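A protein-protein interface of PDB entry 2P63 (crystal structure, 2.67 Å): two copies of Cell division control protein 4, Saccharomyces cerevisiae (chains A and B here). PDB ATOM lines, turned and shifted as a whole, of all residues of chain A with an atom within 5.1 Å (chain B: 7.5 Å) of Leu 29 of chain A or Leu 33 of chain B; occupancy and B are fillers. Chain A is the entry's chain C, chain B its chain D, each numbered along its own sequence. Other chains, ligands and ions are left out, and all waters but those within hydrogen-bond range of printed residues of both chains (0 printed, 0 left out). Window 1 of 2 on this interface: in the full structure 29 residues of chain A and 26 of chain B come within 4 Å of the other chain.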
ATOM      1  N   TYR A  25      10.504  10.916  19.403  1.00  0.00           N
ATOM      2  CA  TYR A  25      10.423  12.374  19.326  1.00  0.00           C
ATOM      3  C   TYR A  25       9.656  12.939  20.517  1.00  0.00           C
ATOM      4  O   TYR A  25      10.040  13.923  21.146  1.00  0.00           O
ATOM      5  CB  TYR A  25       9.759  12.830  18.022  1.00  0.00           C
ATOM      6  CG  TYR A  25       9.483  14.321  18.000  1.00  0.00           C
ATOM      7  CD1 TYR A  25      10.513  15.220  17.746  1.00  0.00           C
ATOM      8  CD2 TYR A  25       8.212  14.833  18.233  1.00  0.00           C
ATOM      9  CE1 TYR A  25      10.271  16.582  17.724  1.00  0.00           C
ATOM     10  CE2 TYR A  25       7.958  16.193  18.214  1.00  0.00           C
ATOM     11  CZ  TYR A  25       8.998  17.060  17.957  1.00  0.00           C
ATOM     12  OH  TYR A  25       8.779  18.417  17.933  1.00  0.00           O
ATOM     13  N   PHE A  26       8.535  12.297  20.824  1.00  0.00           N
ATOM     14  CA  PHE A  26       7.644  12.814  21.860  1.00  0.00           C
ATOM     15  C   PHE A  26       8.220  12.710  23.257  1.00  0.00           C
ATOM     16  O   PHE A  26       8.117  13.699  24.001  1.00  0.00           O
ATOM     17  CB  PHE A  26       6.299  12.077  21.701  1.00  0.00           C
ATOM     18  CG  PHE A  26       6.086  11.738  20.239  1.00  0.00           C
ATOM     19  CD1 PHE A  26       5.893  12.750  19.312  1.00  0.00           C
ATOM     20  CD2 PHE A  26       6.089  10.431  19.789  1.00  0.00           C
ATOM     21  CE1 PHE A  26       5.716  12.449  17.975  1.00  0.00           C
ATOM     22  CE2 PHE A  26       5.910  10.117  18.455  1.00  0.00           C
ATOM     23  CZ  PHE A  26       5.722  11.136  17.539  1.00  0.00           C
ATOM     24  N   LYS A  27       8.825  11.592  23.667  1.00  0.00           N
ATOM     25  CA  LYS A  27       9.388  11.578  25.026  1.00  0.00           C
ATOM     26  C   LYS A  27      10.458  12.661  25.126  1.00  0.00           C
ATOM     27  O   LYS A  27      10.524  13.415  26.095  1.00  0.00           O
ATOM     28  CB  LYS A  27       9.957  10.236  25.448  1.00  0.00           C
ATOM     29  CG  LYS A  27      10.568   9.344  24.392  1.00  0.00           C
ATOM     30  CD  LYS A  27      11.846   8.673  24.873  1.00  0.00           C
ATOM     31  CE  LYS A  27      11.692   7.167  24.998  1.00  0.00           C
ATOM     32  NZ  LYS A  27      12.475   6.413  23.981  1.00  0.00           N
ATOM     33  N   ASN A  28      11.302  12.758  24.098  1.00  0.00           N
ATOM     34  CA  ASN A  28      12.331  13.796  24.132  1.00  0.00           C
ATOM     35  C   ASN A  28      11.687  15.174  24.215  1.00  0.00           C
ATOM     36  O   ASN A  28      12.095  16.030  24.997  1.00  0.00           O
ATOM     37  CB  ASN A  28      13.221  13.722  22.898  1.00  0.00           C
ATOM     38  CG  ASN A  28      14.383  12.765  23.053  1.00  0.00           C
ATOM     39  OD1 ASN A  28      15.485  13.165  23.425  1.00  0.00           O
ATOM     40  ND2 ASN A  28      14.134  11.499  22.748  1.00  0.00           N
ATOM     41  N   LEU A  29      10.673  15.363  23.377  1.00  0.00           N
ATOM     42  CA  LEU A  29       9.944  16.626  23.327  1.00  0.00           C
ATOM     43  C   LEU A  29       9.264  16.886  24.661  1.00  0.00           C
ATOM     44  O   LEU A  29       9.346  17.971  25.236  1.00  0.00           O
ATOM     45  CB  LEU A  29       8.931  16.593  22.185  1.00  0.00           C
ATOM     46  CG  LEU A  29       7.803  17.622  22.220  1.00  0.00           C
ATOM     47  CD1 LEU A  29       8.126  18.806  21.322  1.00  0.00           C
ATOM     48  CD2 LEU A  29       6.484  16.981  21.814  1.00  0.00           C
ATOM     49  N   LEU A  30       8.587  15.858  25.169  1.00  0.00           N
ATOM     50  CA  LEU A  30       7.867  16.010  26.431  1.00  0.00           C
ATOM     51  C   LEU A  30       8.748  16.526  27.554  1.00  0.00           C
ATOM     52  O   LEU A  30       8.282  17.261  28.433  1.00  0.00           O
ATOM     53  CB  LEU A  30       7.225  14.679  26.844  1.00  0.00           C
ATOM     54  CG  LEU A  30       5.786  14.761  27.359  1.00  0.00           C
ATOM     55  CD1 LEU A  30       5.586  13.789  28.511  1.00  0.00           C
ATOM     56  CD2 LEU A  30       5.428  16.177  27.783  1.00  0.00           C
ATOM     57  N   PHE A  31      10.036  16.177  27.586  1.00  0.00           N
ATOM     58  CA  PHE A  31      10.796  16.630  28.770  1.00  0.00           C
ATOM     59  C   PHE A  31      11.555  17.898  28.490  1.00  0.00           C
ATOM     60  O   PHE A  31      11.947  18.670  29.369  1.00  0.00           O
ATOM     61  CB  PHE A  31      11.668  15.451  29.257  1.00  0.00           C
ATOM     62  CG  PHE A  31      10.725  14.349  29.714  1.00  0.00           C
ATOM     63  CD1 PHE A  31      10.402  13.296  28.883  1.00  0.00           C
ATOM     64  CD2 PHE A  31      10.153  14.386  30.975  1.00  0.00           C
ATOM     65  CE1 PHE A  31       9.524  12.300  29.267  1.00  0.00           C
ATOM     66  CE2 PHE A  31       9.269  13.404  31.373  1.00  0.00           C
ATOM     67  CZ  PHE A  31       8.953  12.361  30.525  1.00  0.00           C
ATOM     68  N   ARG A  32      11.776  18.214  27.208  1.00  0.00           N
ATOM     69  CA  ARG A  32      12.406  19.525  26.999  1.00  0.00           C
ATOM     70  C   ARG A  32      11.450  20.628  27.431  1.00  0.00           C
ATOM     71  O   ARG A  32      11.878  21.668  27.932  1.00  0.00           O
ATOM     72  CB  ARG A  32      12.841  19.678  25.546  1.00  0.00           C
ATOM     73  CG  ARG A  32      14.333  19.429  25.349  1.00  0.00           C
ATOM     74  CD  ARG A  32      14.655  19.190  23.885  1.00  0.00           C
ATOM     75  NE  ARG A  32      15.466  17.991  23.697  1.00  0.00           N
ATOM     76  CZ  ARG A  32      16.732  18.017  23.299  1.00  0.00           C
ATOM     77  NH1 ARG A  32      17.322  19.179  23.055  1.00  0.00           N
ATOM     78  NH2 ARG A  32      17.413  16.892  23.147  1.00  0.00           N
ATOM     79  N   LEU A  33      10.148  20.408  27.249  1.00  0.00           N
ATOM     80  CA  LEU A  33       9.152  21.395  27.659  1.00  0.00           C
ATOM     81  C   LEU A  33       9.116  21.512  29.181  1.00  0.00           C
ATOM     82  O   LEU A  33       9.409  22.565  29.737  1.00  0.00           O
ATOM     83  CB  LEU A  33       7.754  21.041  27.155  1.00  0.00           C
ATOM     84  CG  LEU A  33       7.652  20.587  25.698  1.00  0.00           C
ATOM     85  CD1 LEU A  33       6.277  20.006  25.408  1.00  0.00           C
ATOM     86  CD2 LEU A  33       7.980  21.740  24.758  1.00  0.00           C
ATOM     87  N   LEU B   9      17.294  12.211  21.985  1.00  0.00           N
ATOM     88  CA  LEU B   9      17.322  12.885  20.687  1.00  0.00           C
ATOM     89  C   LEU B   9      18.175  14.147  20.800  1.00  0.00           C
ATOM     90  O   LEU B   9      17.752  15.108  21.431  1.00  0.00           O
ATOM     91  CB  LEU B   9      15.926  13.227  20.179  1.00  0.00           C
ATOM     92  CG  LEU B   9      15.150  12.098  19.496  1.00  0.00           C
ATOM     93  CD1 LEU B   9      13.866  12.624  18.875  1.00  0.00           C
ATOM     94  CD2 LEU B   9      16.025  11.413  18.457  1.00  0.00           C
ATOM     95  N   PHE B  14      17.015  17.340  17.454  1.00  0.00           N
ATOM     96  CA  PHE B  14      15.753  17.875  17.937  1.00  0.00           C
ATOM     97  C   PHE B  14      15.423  19.201  17.257  1.00  0.00           C
ATOM     98  O   PHE B  14      14.279  19.440  16.869  1.00  0.00           O
ATOM     99  CB  PHE B  14      15.796  18.082  19.451  1.00  0.00           C
ATOM    100  CG  PHE B  14      14.489  18.544  20.038  1.00  0.00           C
ATOM    101  CD1 PHE B  14      14.374  19.794  20.618  1.00  0.00           C
ATOM    102  CD2 PHE B  14      13.375  17.722  20.005  1.00  0.00           C
ATOM    103  CE1 PHE B  14      13.171  20.214  21.153  1.00  0.00           C
ATOM    104  CE2 PHE B  14      12.170  18.131  20.538  1.00  0.00           C
ATOM    105  CZ  PHE B  14      12.069  19.380  21.119  1.00  0.00           C
ATOM    106  N   ASN B  18      12.300  19.963  14.369  1.00  0.00           N
ATOM    107  CA  ASN B  18      11.348  21.011  14.710  1.00  0.00           C
ATOM    108  C   ASN B  18      11.392  22.197  13.769  1.00  0.00           C
ATOM    109  O   ASN B  18      10.349  22.808  13.497  1.00  0.00           O
ATOM    110  CB  ASN B  18      11.584  21.473  16.159  1.00  0.00           C
ATOM    111  CG  ASN B  18      11.273  20.332  17.113  1.00  0.00           C
ATOM    112  OD1 ASN B  18      10.466  19.463  16.778  1.00  0.00           O
ATOM    113  ND2 ASN B  18      11.913  20.326  18.276  1.00  0.00           N
ATOM    114  N   LEU B  21       9.203  21.560  11.186  1.00  0.00           N
ATOM    115  CA  LEU B  21       7.846  21.268  11.649  1.00  0.00           C
ATOM    116  C   LEU B  21       6.993  22.510  11.403  1.00  0.00           C
ATOM    117  O   LEU B  21       7.540  23.613  11.303  1.00  0.00           O
ATOM    118  CB  LEU B  21       7.824  20.855  13.113  1.00  0.00           C
ATOM    119  CG  LEU B  21       7.963  19.367  13.434  1.00  0.00           C
ATOM    120  CD1 LEU B  21       8.168  19.149  14.926  1.00  0.00           C
ATOM    121  CD2 LEU B  21       6.747  18.586  12.951  1.00  0.00           C
ATOM    122  N   TYR B  25       1.841  23.322  14.104  1.00  0.00           N
ATOM    123  CA  TYR B  25       2.024  22.058  14.815  1.00  0.00           C
ATOM    124  C   TYR B  25       2.335  22.303  16.289  1.00  0.00           C
ATOM    125  O   TYR B  25       2.131  21.439  17.142  1.00  0.00           O
ATOM    126  CB  TYR B  25       3.137  21.236  14.165  1.00  0.00           C
ATOM    127  CG  TYR B  25       3.438  19.900  14.804  1.00  0.00           C
ATOM    128  CD1 TYR B  25       4.404  19.784  15.795  1.00  0.00           C
ATOM    129  CD2 TYR B  25       2.774  18.737  14.426  1.00  0.00           C
ATOM    130  CE1 TYR B  25       4.696  18.572  16.391  1.00  0.00           C
ATOM    131  CE2 TYR B  25       3.056  17.518  15.014  1.00  0.00           C
ATOM    132  CZ  TYR B  25       4.019  17.438  15.997  1.00  0.00           C
ATOM    133  OH  TYR B  25       4.319  16.237  16.599  1.00  0.00           O
ATOM    134  N   PHE B  26       2.838  23.497  16.579  1.00  0.00           N
ATOM    135  CA  PHE B  26       3.281  23.854  17.917  1.00  0.00           C
ATOM    136  C   PHE B  26       2.201  24.516  18.752  1.00  0.00           C
ATOM    137  O   PHE B  26       2.521  25.136  19.769  1.00  0.00           O
ATOM    138  CB  PHE B  26       4.491  24.796  17.789  1.00  0.00           C
ATOM    139  CG  PHE B  26       5.627  24.125  17.054  1.00  0.00           C
ATOM    140  CD1 PHE B  26       6.185  22.961  17.562  1.00  0.00           C
ATOM    141  CD2 PHE B  26       6.124  24.642  15.874  1.00  0.00           C
ATOM    142  CE1 PHE B  26       7.223  22.320  16.912  1.00  0.00           C
ATOM    143  CE2 PHE B  26       7.165  24.013  15.216  1.00  0.00           C
ATOM    144  CZ  PHE B  26       7.715  22.854  15.735  1.00  0.00           C
ATOM    145  N   ASN B  28      -0.733  24.256  21.185  1.00  0.00           N
ATOM    146  CA  ASN B  28      -1.320  23.505  22.281  1.00  0.00           C
ATOM    147  C   ASN B  28      -1.148  22.002  22.098  1.00  0.00           C
ATOM    148  O   ASN B  28      -2.016  21.210  22.469  1.00  0.00           O
ATOM    149  CB  ASN B  28      -2.793  23.906  22.440  1.00  0.00           C
ATOM    150  CG  ASN B  28      -2.938  25.421  22.482  1.00  0.00           C
ATOM    151  OD1 ASN B  28      -2.226  26.114  23.216  1.00  0.00           O
ATOM    152  ND2 ASN B  28      -3.860  25.946  21.682  1.00  0.00           N
ATOM    153  N   LEU B  29       0.000  21.635  21.541  1.00  0.00           N
ATOM    154  CA  LEU B  29       0.505  20.280  21.437  1.00  0.00           C
ATOM    155  C   LEU B  29       0.175  19.447  22.680  1.00  0.00           C
ATOM    156  O   LEU B  29      -0.206  18.287  22.547  1.00  0.00           O
ATOM    157  CB  LEU B  29       2.024  20.288  21.293  1.00  0.00           C
ATOM    158  CG  LEU B  29       2.649  19.782  20.000  1.00  0.00           C
ATOM    159  CD1 LEU B  29       4.095  20.253  19.931  1.00  0.00           C
ATOM    160  CD2 LEU B  29       2.562  18.269  19.884  1.00  0.00           C
ATOM    161  N   LEU B  30       0.349  20.061  23.841  1.00  0.00           N
ATOM    162  CA  LEU B  30       0.182  19.492  25.165  1.00  0.00           C
ATOM    163  C   LEU B  30      -1.205  18.933  25.423  1.00  0.00           C
ATOM    164  O   LEU B  30      -1.358  17.879  26.051  1.00  0.00           O
ATOM    165  CB  LEU B  30       0.509  20.555  26.226  1.00  0.00           C
ATOM    166  CG  LEU B  30       1.876  20.408  26.902  1.00  0.00           C
ATOM    167  CD1 LEU B  30       2.953  20.110  25.869  1.00  0.00           C
ATOM    168  CD2 LEU B  30       2.207  21.658  27.700  1.00  0.00           C
ATOM    169  N   PHE B  31      -2.263  19.602  24.960  1.00  0.00           N
ATOM    170  CA  PHE B  31      -3.576  18.967  25.136  1.00  0.00           C
ATOM    171  C   PHE B  31      -3.685  17.804  24.155  1.00  0.00           C
ATOM    172  O   PHE B  31      -4.185  16.736  24.500  1.00  0.00           O
ATOM    173  CB  PHE B  31      -4.717  19.956  24.948  1.00  0.00           C
ATOM    174  CG  PHE B  31      -5.997  19.636  25.675  1.00  0.00           C
ATOM    175  CD1 PHE B  31      -6.614  18.400  25.547  1.00  0.00           C
ATOM    176  CD2 PHE B  31      -6.599  20.578  26.497  1.00  0.00           C
ATOM    177  CE1 PHE B  31      -7.790  18.106  26.210  1.00  0.00           C
ATOM    178  CE2 PHE B  31      -7.777  20.296  27.165  1.00  0.00           C
ATOM    179  CZ  PHE B  31      -8.378  19.058  27.024  1.00  0.00           C
ATOM    180  N   ARG B  32      -3.207  18.013  22.926  1.00  0.00           N
ATOM    181  CA  ARG B  32      -3.247  16.910  21.963  1.00  0.00           C
ATOM    182  C   ARG B  32      -2.454  15.738  22.544  1.00  0.00           C
ATOM    183  O   ARG B  32      -2.973  14.634  22.664  1.00  0.00           O
ATOM    184  CB  ARG B  32      -2.697  17.299  20.600  1.00  0.00           C
ATOM    185  CG  ARG B  32      -3.327  18.507  19.934  1.00  0.00           C
ATOM    186  CD  ARG B  32      -3.649  18.230  18.472  1.00  0.00           C
ATOM    187  NE  ARG B  32      -3.478  19.407  17.630  1.00  0.00           N
ATOM    188  CZ  ARG B  32      -4.013  19.620  16.438  1.00  0.00           C
ATOM    189  NH1 ARG B  32      -4.807  18.731  15.859  1.00  0.00           N
ATOM    190  NH2 ARG B  32      -3.750  20.757  15.801  1.00  0.00           N
ATOM    191  N   LEU B  33      -1.213  16.032  22.906  1.00  0.00           N
ATOM    192  CA  LEU B  33      -0.324  15.066  23.538  1.00  0.00           C
ATOM    193  C   LEU B  33      -1.033  14.425  24.721  1.00  0.00           C
ATOM    194  O   LEU B  33      -1.354  13.237  24.680  1.00  0.00           O
ATOM    195  CB  LEU B  33       0.985  15.725  23.968  1.00  0.00           C
ATOM    196  CG  LEU B  33       1.965  16.046  22.835  1.00  0.00           C
ATOM    197  CD1 LEU B  33       3.256  16.641  23.375  1.00  0.00           C
ATOM    198  CD2 LEU B  33       2.265  14.802  22.012  1.00  0.00           C
ATOM    199  N   VAL B  34      -1.304  15.200  25.764  1.00  0.00           N
ATOM    200  CA  VAL B  34      -2.026  14.681  26.924  1.00  0.00           C
ATOM    201  C   VAL B  34      -3.318  13.976  26.525  1.00  0.00           C
ATOM    202  O   VAL B  34      -3.739  13.016  27.177  1.00  0.00           O
ATOM    203  CB  VAL B  34      -2.341  15.799  27.930  1.00  0.00           C
ATOM    204  CG1 VAL B  34      -3.244  15.268  29.031  1.00  0.00           C
ATOM    205  CG2 VAL B  34      -1.049  16.361  28.506  1.00  0.00           C
ATOM    206  N   ALA B  35      -3.936  14.435  25.441  1.00  0.00           N
ATOM    207  CA  ALA B  35      -5.047  13.706  24.842  1.00  0.00           C
ATOM    208  C   ALA B  35      -4.553  12.357  24.317  1.00  0.00           C
ATOM    209  O   ALA B  35      -5.183  11.331  24.565  1.00  0.00           O
ATOM    210  CB  ALA B  35      -5.696  14.511  23.731  1.00  0.00           C
ATOM    211  N   ASN B  36      -3.436  12.368  23.604  1.00  0.00           N
ATOM    212  CA  ASN B  36      -2.817  11.186  23.021  1.00  0.00           C
ATOM    213  C   ASN B  36      -1.831  10.564  24.012  1.00  0.00           C
ATOM    214  O   ASN B  36      -0.718  10.176  23.660  1.00  0.00           O
ATOM    215  CB  ASN B  36      -2.102  11.525  21.715  1.00  0.00           C
ATOM    216  CG  ASN B  36      -3.064  11.748  20.564  1.00  0.00           C
ATOM    217  OD1 ASN B  36      -4.219  11.322  20.607  1.00  0.00           O
ATOM    218  ND2 ASN B  36      -2.584  12.421  19.523  1.00  0.00           N
ATOM    219  N   MET B  37      -2.310  10.524  25.246  1.00  0.00           N
ATOM    220  CA  MET B  37      -1.550  10.099  26.416  1.00  0.00           C
ATOM    221  C   MET B  37      -2.463   9.384  27.410  1.00  0.00           C
ATOM    222  O   MET B  37      -3.046  10.016  28.289  1.00  0.00           O
ATOM    223  CB  MET B  37      -0.895  11.317  27.062  1.00  0.00           C
ATOM    224  CG  MET B  37      -0.027  10.929  28.257  1.00  0.00           C
ATOM    225  SD  MET B  37       0.614  12.509  29.206  1.00  0.00           S
ATOM    226  CE  MET B  37       1.214  13.279  27.524  1.00  0.00           C
ATOM    227  N   ASP B  38      -2.575   8.073  27.249  1.00  0.00           N
ATOM    228  CA  ASP B  38      -3.391   7.231  28.110  1.00  0.00           C
ATOM    229  C   ASP B  38      -3.082   7.483  29.582  1.00  0.00           C
ATOM    230  O   ASP B  38      -2.036   8.046  29.907  1.00  0.00           O
ATOM    231  CB  ASP B  38      -3.175   5.752  27.777  1.00  0.00           C
ATOM    232  CG  ASP B  38      -2.456   5.015  28.890  1.00  0.00           C
ATOM    233  OD1 ASP B  38      -1.246   4.756  28.739  1.00  0.00           O
ATOM    234  OD2 ASP B  38      -3.104   4.703  29.913  1.00  0.00           O
ATOM    235  N   GLU B  41       0.651   6.753  31.190  1.00  0.00           N
ATOM    236  CA  GLU B  41       1.560   7.862  30.933  1.00  0.00           C
ATOM    237  C   GLU B  41       1.199   9.059  31.807  1.00  0.00           C
ATOM    238  O   GLU B  41       2.014   9.615  32.535  1.00  0.00           O
ATOM    239  CB  GLU B  41       1.494   8.255  29.455  1.00  0.00           C
ATOM    240  CG  GLU B  41       1.618   7.073  28.509  1.00  0.00           C
ATOM    241  CD  GLU B  41       0.890   7.251  27.193  1.00  0.00           C
ATOM    242  OE1 GLU B  41       1.523   7.650  26.188  1.00  0.00           O
ATOM    243  OE2 GLU B  41      -0.330   6.980  27.159  1.00  0.00           O
ATOM    244  N   LEU B  42      -0.069   9.420  31.695  1.00  0.00           N
ATOM    245  CA  LEU B  42      -0.705  10.502  32.414  1.00  0.00           C
ATOM    246  C   LEU B  42      -0.282  10.530  33.872  1.00  0.00           C
ATOM    247  O   LEU B  42       0.139  11.539  34.441  1.00  0.00           O
ATOM    248  CB  LEU B  42      -2.225  10.327  32.315  1.00  0.00           C
ATOM    249  CG  LEU B  42      -3.031  11.404  31.590  1.00  0.00           C
ATOM    250  CD1 LEU B  42      -2.237  12.021  30.449  1.00  0.00           C
ATOM    251  CD2 LEU B  42      -4.350  10.824  31.089  1.00  0.00           C
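CA of Tyr 25 of chain A touches CD1 of Leu 9 of chain B, at 3.5 Å. CE1 of Tyr 25 of chain A touches CE2 of Phe 14 of chain B, 3.7 Å away. Tyr 25 of chain A touches Leu 21 of chain B (OH to CD1, 3.2 Å). Tyr 25 of chain B touches Tyr 25 of chain A (OH to CE2, 3.98 Å). Leu 29 of chain A touches Phe 14 of chain B (CA to CE2, 3.9 Å). CD2 of Leu 29 of chain A touches CD1 of Leu 33 of chain B, 3.6 Å away. Phe 14 of chain B touches Arg 32 of chain A (CE1 to CD, 3.3 Å). CD1 of Leu 30 of chain B touches CD1 of Leu 33 of chain A (3.4 Å).
Leu 29 of chain A touches just these residues of chain B: Phe 14 and Leu 33. Leu 30 of chain A touches none of the printed residues of chain B. Of the printed residues of chain A, Tyr 25 of chain B touches Tyr 25 (3.98 Å). Leu 29 of chain B touches none of the printed residues of chain A. Printed residues of chain A within 4 Å of Leu 30 of chain B: Leu 33. Leu 33 of chain B touches one residue of chain A. The nearest residue of chain B that does not touch Leu 29 of chain A is Leu 29 of chain B (4.5 Å).
Of the 19 printed residues of chain B, 7 touch a printed residue of chain A. Hydrophobic or aromatic side chains of chain B within 4 Å of the printed part of chain A: Leu 9, Phe 14, Leu 21, Tyr 25, Leu 30 and Leu 33. Of the 9 printed residues of chain A, 5 touch a printed residue of chain B. Printed residues of chain A that touch a printed residue of chain B: Tyr 25, Asn 28, Leu 29, Arg 32 and Leu 33. Hydrophobic or aromatic side chains of chain A within 4 Å of the printed part of chain B: Tyr 25, Leu 29 and Leu 33. Among the printed residues, 11 pairs touch across the chains.
The side-chain amide nitrogen (ND2) of Asn 18 of chain B lies within hydrogen-bond range of the backbone carbonyl oxygen (O) of Phe 14 of chain B.
The side-chain amide oxygen of Asn 28 of chain A sits at hydrogen-bond distance from the backbone NH of Leu 9 of chain B (2.5 Å). The side-chain amide oxygen (OD1) of Asn 18 of chain B lies close to the side-chain hydroxyl (OH) of Tyr 25 of chain A, 2.3 Å away. The backbone carbonyl oxygen (O) of Leu 9 of chain B is in hydrogen-bond range of the guanidinium group (NH2) of Arg 32 of chain A, at 2.5 Å.
Tyr 25 of chain A touches its own counterpart, Tyr 25 of chain B. Leu 29 of chain A touches Leu 33 of chain B, but with the chains exchanged Leu 33 of chain A does not touch Leu 29 of chain B (5.9 Å). Leu 33 of chain A touches Leu 30 of chain B, but with the chains exchanged Leu 30 of chain A does not touch Leu 33 of chain B (4.9 Å). Of the 11 pairs that touch across the chains among the printed residues, 1 has its exchanged pair printed and touching as well.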
